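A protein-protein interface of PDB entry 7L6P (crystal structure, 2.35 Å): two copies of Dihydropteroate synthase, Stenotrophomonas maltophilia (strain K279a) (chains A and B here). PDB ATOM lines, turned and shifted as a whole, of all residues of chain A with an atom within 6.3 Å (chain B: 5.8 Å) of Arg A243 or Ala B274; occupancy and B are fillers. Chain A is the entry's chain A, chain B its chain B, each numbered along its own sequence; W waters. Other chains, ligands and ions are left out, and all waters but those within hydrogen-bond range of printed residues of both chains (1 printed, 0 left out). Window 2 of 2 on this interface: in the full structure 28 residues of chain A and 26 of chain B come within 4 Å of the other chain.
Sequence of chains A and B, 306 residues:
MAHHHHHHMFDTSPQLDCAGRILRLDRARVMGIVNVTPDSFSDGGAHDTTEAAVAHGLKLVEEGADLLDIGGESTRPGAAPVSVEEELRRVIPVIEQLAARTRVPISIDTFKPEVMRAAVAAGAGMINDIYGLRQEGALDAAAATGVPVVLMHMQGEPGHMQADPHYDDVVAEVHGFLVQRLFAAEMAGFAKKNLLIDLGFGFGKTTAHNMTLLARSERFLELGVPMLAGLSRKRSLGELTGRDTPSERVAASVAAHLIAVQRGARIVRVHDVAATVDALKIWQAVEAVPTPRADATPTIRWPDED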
ATOM      1  N   ARG A 235      20.101   3.886  -2.686  1.00  0.00           N
ATOM      2  CA  ARG A 235      19.362   4.581  -3.748  1.00  0.00           C
ATOM      3  C   ARG A 235      18.039   5.121  -3.237  1.00  0.00           C
ATOM      4  O   ARG A 235      17.581   6.176  -3.693  1.00  0.00           O
ATOM      5  CB  ARG A 235      19.124   3.632  -4.926  1.00  0.00           C
ATOM      6  CG  ARG A 235      18.120   4.106  -5.989  1.00  0.00           C
ATOM      7  CD  ARG A 235      17.399   2.877  -6.633  1.00  0.00           C
ATOM      8  NE  ARG A 235      16.566   2.174  -5.656  1.00  0.00           N
ATOM      9  CZ  ARG A 235      15.272   2.412  -5.488  1.00  0.00           C
ATOM     10  NH1 ARG A 235      14.640   3.324  -6.218  1.00  0.00           N
ATOM     11  NH2 ARG A 235      14.591   1.713  -4.584  1.00  0.00           N
ATOM     12  N   LEU A 237      17.503   6.392  -0.350  1.00  0.00           N
ATOM     13  CA  LEU A 237      17.772   7.714   0.230  1.00  0.00           C
ATOM     14  C   LEU A 237      17.886   8.778  -0.863  1.00  0.00           C
ATOM     15  O   LEU A 237      17.464   9.930  -0.677  1.00  0.00           O
ATOM     16  CB  LEU A 237      19.040   7.679   1.089  1.00  0.00           C
ATOM     17  CG  LEU A 237      19.134   6.644   2.223  1.00  0.00           C
ATOM     18  CD1 LEU A 237      20.396   6.895   3.014  1.00  0.00           C
ATOM     19  CD2 LEU A 237      17.936   6.719   3.159  1.00  0.00           C
ATOM     20  N   GLY A 238      18.460   8.416  -2.008  1.00  0.00           N
ATOM     21  CA  GLY A 238      18.515   9.368  -3.102  1.00  0.00           C
ATOM     22  C   GLY A 238      17.136   9.667  -3.657  1.00  0.00           C
ATOM     23  O   GLY A 238      16.829  10.806  -4.010  1.00  0.00           O
ATOM     24  N   GLU A 239      16.272   8.657  -3.702  1.00  0.00           N
ATOM     25  CA  GLU A 239      14.914   8.879  -4.179  1.00  0.00           C
ATOM     26  C   GLU A 239      14.150   9.789  -3.229  1.00  0.00           C
ATOM     27  O   GLU A 239      13.388  10.656  -3.669  1.00  0.00           O
ATOM     28  CB  GLU A 239      14.206   7.540  -4.375  1.00  0.00           C
ATOM     29  CG  GLU A 239      12.785   7.624  -4.897  1.00  0.00           C
ATOM     30  CD  GLU A 239      12.305   6.279  -5.455  1.00  0.00           C
ATOM     31  OE1 GLU A 239      12.890   5.238  -5.068  1.00  0.00           O
ATOM     32  OE2 GLU A 239      11.369   6.269  -6.298  1.00  0.00           O
ATOM     33  N   LEU A 240      14.351   9.621  -1.928  1.00  0.00           N
ATOM     34  CA  LEU A 240      13.652  10.462  -0.958  1.00  0.00           C
ATOM     35  C   LEU A 240      14.146  11.911  -0.978  1.00  0.00           C
ATOM     36  O   LEU A 240      13.349  12.843  -0.792  1.00  0.00           O
ATOM     37  CB  LEU A 240      13.804   9.847   0.436  1.00  0.00           C
ATOM     38  CG  LEU A 240      12.933   8.604   0.645  1.00  0.00           C
ATOM     39  CD1 LEU A 240      13.368   7.797   1.855  1.00  0.00           C
ATOM     40  CD2 LEU A 240      11.493   9.023   0.819  1.00  0.00           C
ATOM     41  N   THR A 241      15.441  12.126  -1.234  1.00  0.00           N
ATOM     42  CA  THR A 241      16.049  13.451  -1.173  1.00  0.00           C
ATOM     43  C   THR A 241      16.317  14.098  -2.530  1.00  0.00           C
ATOM     44  O   THR A 241      16.496  15.325  -2.591  1.00  0.00           O
ATOM     45  CB  THR A 241      17.390  13.367  -0.437  1.00  0.00           C
ATOM     46  OG1 THR A 241      18.243  12.445  -1.136  1.00  0.00           O
ATOM     47  CG2 THR A 241      17.200  12.905   0.998  1.00  0.00           C
ATOM     48  N   GLY A 242      16.302  13.344  -3.622  1.00  0.00           N
ATOM     49  CA  GLY A 242      16.688  13.907  -4.896  1.00  0.00           C
ATOM     50  C   GLY A 242      18.173  13.880  -5.185  1.00  0.00           C
ATOM     51  O   GLY A 242      18.589  14.459  -6.184  1.00  0.00           O
ATOM     52  N   ARG A 243      18.973  13.153  -4.402  1.00  0.00           N
ATOM     53  CA  ARG A 243      20.427  13.118  -4.571  1.00  0.00           C
ATOM     54  C   ARG A 243      20.856  11.950  -5.442  1.00  0.00           C
ATOM     55  O   ARG A 243      20.836  10.797  -4.995  1.00  0.00           O
ATOM     56  CB  ARG A 243      21.141  13.007  -3.232  1.00  0.00           C
ATOM     57  CG  ARG A 243      20.699  13.998  -2.227  1.00  0.00           C
ATOM     58  CD  ARG A 243      21.358  15.325  -2.441  1.00  0.00           C
ATOM     59  NE  ARG A 243      20.817  16.268  -1.473  1.00  0.00           N
ATOM     60  CZ  ARG A 243      20.837  17.584  -1.609  1.00  0.00           C
ATOM     61  NH1 ARG A 243      21.415  18.164  -2.650  1.00  0.00           N
ATOM     62  NH2 ARG A 243      20.267  18.336  -0.668  1.00  0.00           N
ATOM     63  N   ASP A 244      21.306  12.247  -6.659  1.00  0.00           N
ATOM     64  CA  ASP A 244      21.790  11.174  -7.520  1.00  0.00           C
ATOM     65  C   ASP A 244      23.153  10.643  -7.083  1.00  0.00           C
ATOM     66  O   ASP A 244      23.430   9.456  -7.263  1.00  0.00           O
ATOM     67  CB  ASP A 244      21.887  11.649  -8.970  1.00  0.00           C
ATOM     68  CG  ASP A 244      20.745  11.163  -9.829  1.00  0.00           C
ATOM     69  OD1 ASP A 244      19.820  10.532  -9.318  1.00  0.00           O
ATOM     70  OD2 ASP A 244      20.849  11.304 -11.051  1.00  0.00           O
ATOM     71  N   THR A 245      24.025  11.494  -6.530  1.00  0.00           N
ATOM     72  CA  THR A 245      25.368  11.029  -6.172  1.00  0.00           C
ATOM     73  C   THR A 245      25.324  10.314  -4.819  1.00  0.00           C
ATOM     74  O   THR A 245      24.806  10.874  -3.848  1.00  0.00           O
ATOM     75  CB  THR A 245      26.344  12.210  -6.141  1.00  0.00           C
ATOM     76  OG1 THR A 245      26.221  12.970  -7.360  1.00  0.00           O
ATOM     77  CG2 THR A 245      27.794  11.740  -6.023  1.00  0.00           C
ATOM     78  N   PRO A 246      25.826   9.078  -4.718  1.00  0.00           N
ATOM     79  CA  PRO A 246      25.748   8.375  -3.420  1.00  0.00           C
ATOM     80  C   PRO A 246      26.519   9.073  -2.314  1.00  0.00           C
ATOM     81  O   PRO A 246      26.090   9.053  -1.151  1.00  0.00           O
ATOM     82  CB  PRO A 246      26.332   6.987  -3.730  1.00  0.00           C
ATOM     83  CG  PRO A 246      26.107   6.808  -5.205  1.00  0.00           C
ATOM     84  CD  PRO A 246      26.298   8.197  -5.806  1.00  0.00           C
ATOM     85  N   GLU A 248      26.746  12.186  -1.926  1.00  0.00           N
ATOM     86  CA  GLU A 248      25.915  13.317  -1.541  1.00  0.00           C
ATOM     87  C   GLU A 248      24.815  12.931  -0.554  1.00  0.00           C
ATOM     88  O   GLU A 248      23.989  13.785  -0.219  1.00  0.00           O
ATOM     89  CB  GLU A 248      25.273  13.936  -2.788  1.00  0.00           C
ATOM     90  CG  GLU A 248      26.191  14.900  -3.575  1.00  0.00           C
ATOM     91  CD  GLU A 248      25.607  15.319  -4.907  1.00  0.00           C
ATOM     92  OE1 GLU A 248      24.514  14.824  -5.297  1.00  0.00           O
ATOM     93  OE2 GLU A 248      26.250  16.165  -5.568  1.00  0.00           O
ATOM     94  N   ARG A 249      24.780  11.679  -0.084  1.00  0.00           N
ATOM     95  CA  ARG A 249      23.685  11.177   0.738  1.00  0.00           C
ATOM     96  C   ARG A 249      24.081  10.943   2.199  1.00  0.00           C
ATOM     97  O   ARG A 249      23.459  10.122   2.879  1.00  0.00           O
ATOM     98  CB  ARG A 249      23.130   9.883   0.145  1.00  0.00           C
ATOM     99  CG  ARG A 249      22.538  10.016  -1.238  1.00  0.00           C
ATOM    100  CD  ARG A 249      22.254   8.653  -1.863  1.00  0.00           C
ATOM    101  NE  ARG A 249      21.800   8.788  -3.236  1.00  0.00           N
ATOM    102  CZ  ARG A 249      21.768   7.811  -4.135  1.00  0.00           C
ATOM    103  NH1 ARG A 249      22.143   6.574  -3.838  1.00  0.00           N
ATOM    104  NH2 ARG A 249      21.336   8.079  -5.362  1.00  0.00           N
ATOM    105  N   ALA A 251      24.072  13.093   4.992  1.00  0.00           N
ATOM    106  CA  ALA A 251      23.092  13.582   5.957  1.00  0.00           C
ATOM    107  C   ALA A 251      21.875  12.668   6.030  1.00  0.00           C
ATOM    108  O   ALA A 251      21.328  12.452   7.106  1.00  0.00           O
ATOM    109  CB  ALA A 251      22.666  15.017   5.621  1.00  0.00           C
ATOM    110  N   GLU B  63      18.175  25.441  -1.479  1.00  0.00           N
ATOM    111  CA  GLU B  63      18.492  24.210  -0.755  1.00  0.00           C
ATOM    112  C   GLU B  63      17.311  23.665   0.041  1.00  0.00           C
ATOM    113  O   GLU B  63      17.402  22.556   0.589  1.00  0.00           O
ATOM    114  CB  GLU B  63      19.675  24.413   0.195  1.00  0.00           C
ATOM    115  CG  GLU B  63      21.018  24.704  -0.462  1.00  0.00           C
ATOM    116  CD  GLU B  63      22.208  24.590   0.511  1.00  0.00           C
ATOM    117  OE1 GLU B  63      21.996  24.399   1.747  1.00  0.00           O
ATOM    118  OE2 GLU B  63      23.363  24.728   0.036  1.00  0.00           O
ATOM    119  N   ASP B 272      23.325  24.508   8.079  1.00  0.00           N
ATOM    120  CA  ASP B 272      23.401  23.437   7.077  1.00  0.00           C
ATOM    121  C   ASP B 272      21.983  23.065   6.641  1.00  0.00           C
ATOM    122  O   ASP B 272      21.367  22.107   7.135  1.00  0.00           O
ATOM    123  CB  ASP B 272      24.124  22.220   7.654  1.00  0.00           C
ATOM    124  CG  ASP B 272      25.444  22.582   8.311  1.00  0.00           C
ATOM    125  OD1 ASP B 272      26.412  22.810   7.558  1.00  0.00           O
ATOM    126  OD2 ASP B 272      25.500  22.663   9.573  1.00  0.00           O
ATOM    127  N   VAL B 273      21.469  23.844   5.685  1.00  0.00           N
ATOM    128  CA  VAL B 273      20.071  23.722   5.281  1.00  0.00           C
ATOM    129  C   VAL B 273      19.839  22.436   4.499  1.00  0.00           C
ATOM    130  O   VAL B 273      18.939  21.660   4.830  1.00  0.00           O
ATOM    131  CB  VAL B 273      19.634  24.963   4.481  1.00  0.00           C
ATOM    132  CG1 VAL B 273      18.318  24.697   3.733  1.00  0.00           C
ATOM    133  CG2 VAL B 273      19.461  26.126   5.419  1.00  0.00           C
ATOM    134  N   ALA B 274      20.607  22.210   3.426  1.00  0.00           N
ATOM    135  CA  ALA B 274      20.374  21.038   2.587  1.00  0.00           C
ATOM    136  C   ALA B 274      20.451  19.752   3.403  1.00  0.00           C
ATOM    137  O   ALA B 274      19.654  18.833   3.212  1.00  0.00           O
ATOM    138  CB  ALA B 274      21.376  21.000   1.428  1.00  0.00           C
ATOM    139  N   ALA B 275      21.389  19.695   4.339  1.00  0.00           N
ATOM    140  CA  ALA B 275      21.565  18.524   5.177  1.00  0.00           C
ATOM    141  C   ALA B 275      20.377  18.337   6.127  1.00  0.00           C
ATOM    142  O   ALA B 275      19.886  17.215   6.316  1.00  0.00           O
ATOM    143  CB  ALA B 275      22.882  18.658   5.933  1.00  0.00           C
ATOM    144  N   THR B 276      19.903  19.425   6.732  1.00  0.00           N
ATOM    145  CA  THR B 276      18.737  19.338   7.598  1.00  0.00           C
ATOM    146  C   THR B 276      17.502  18.957   6.796  1.00  0.00           C
ATOM    147  O   THR B 276      16.688  18.145   7.256  1.00  0.00           O
ATOM    148  CB  THR B 276      18.510  20.674   8.305  1.00  0.00           C
ATOM    149  OG1 THR B 276      19.735  21.117   8.897  1.00  0.00           O
ATOM    150  CG2 THR B 276      17.456  20.547   9.408  1.00  0.00           C
ATOM    151  N   VAL B 277      17.344  19.558   5.602  1.00  0.00           N
ATOM    152  CA  VAL B 277      16.222  19.246   4.711  1.00  0.00           C
ATOM    153  C   VAL B 277      16.205  17.763   4.353  1.00  0.00           C
ATOM    154  O   VAL B 277      15.153  17.117   4.396  1.00  0.00           O
ATOM    155  CB  VAL B 277      16.278  20.121   3.445  1.00  0.00           C
ATOM    156  CG1 VAL B 277      15.446  19.488   2.272  1.00  0.00           C
ATOM    157  CG2 VAL B 277      15.779  21.527   3.754  1.00  0.00           C
ATOM    158  N   ASP B 278      17.365  17.215   3.969  1.00  0.00           N
ATOM    159  CA  ASP B 278      17.457  15.804   3.609  1.00  0.00           C
ATOM    160  C   ASP B 278      17.039  14.917   4.775  1.00  0.00           C
ATOM    161  O   ASP B 278      16.234  13.993   4.611  1.00  0.00           O
ATOM    162  CB  ASP B 278      18.889  15.460   3.199  1.00  0.00           C
ATOM    163  CG  ASP B 278      19.274  15.965   1.815  1.00  0.00           C
ATOM    164  OD1 ASP B 278      18.500  16.673   1.095  1.00  0.00           O
ATOM    165  OD2 ASP B 278      20.413  15.623   1.434  1.00  0.00           O
ATOM    166  N   ALA B 279      17.548  15.210   5.977  1.00  0.00           N
ATOM    167  CA  ALA B 279      17.188  14.431   7.152  1.00  0.00           C
ATOM    168  C   ALA B 279      15.697  14.497   7.421  1.00  0.00           C
ATOM    169  O   ALA B 279      15.081  13.481   7.744  1.00  0.00           O
ATOM    170  CB  ALA B 279      17.967  14.917   8.370  1.00  0.00           C
HETATM  171  O   HOH W   1      21.745  13.811   2.405  1.00  0.00           O
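No position is printed for both chains. Of the 4 pairs that touch across the chains among the printed residues, none has its exchanged pair printed and touching as well.
OD1 of Asp B278 is in salt-bridge range of NH2 of Arg A243.
Among the printed residues, pairs that only touch across the chains: Arg A243 with Ala B274, Ala A251 with Ala B275 and Thr A241 with Asp B278.
Among the printed residues, 4 pairs touch across the chains.
Printed residues of chain B within 4 Å of Thr A241: Asp B278. Arg A243 touches just these residues of chain B: Ala B274 and Asp B278. Arg A249 touches none of the printed residues of chain B. Of the printed residues of chain B, Ala A251 touches Ala B275 (3.6 Å). Ala B274 touches just one residue of chain A: Arg A243 (3.6 Å). Printed residues of chain A within 4 Å of Ala B275: Ala A251 (3.6 Å). Printed residues of chain A within 4 Å of Asp B278: Thr A241 (3.8 Å) and Arg A243 (3.0 Å). The nearest residue of chain A that does not touch Ala B274 is Ala A251 (5.4 Å).
OG1 of Thr A241 sits close to N of Arg A243. The guanidinium group (NH2) of Arg A249 is in hydrogen-bond range of the backbone carbonyl oxygen (O) of Arg A243 (2.8 Å). N of Ala B274 lies within hydrogen-bond range of OE1 of Glu B63, at 3.1 Å. O of Gly A238 is in hydrogen-bond range of N of Arg A243, at 3.2 Å. O of Leu A237 lies within hydrogen-bond range of OG1 of Thr A241, 2.7 Å away.
Water W1 bridges OD2 of Asp B278 (2.4 Å) and O of Glu A248 (3.5 Å).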
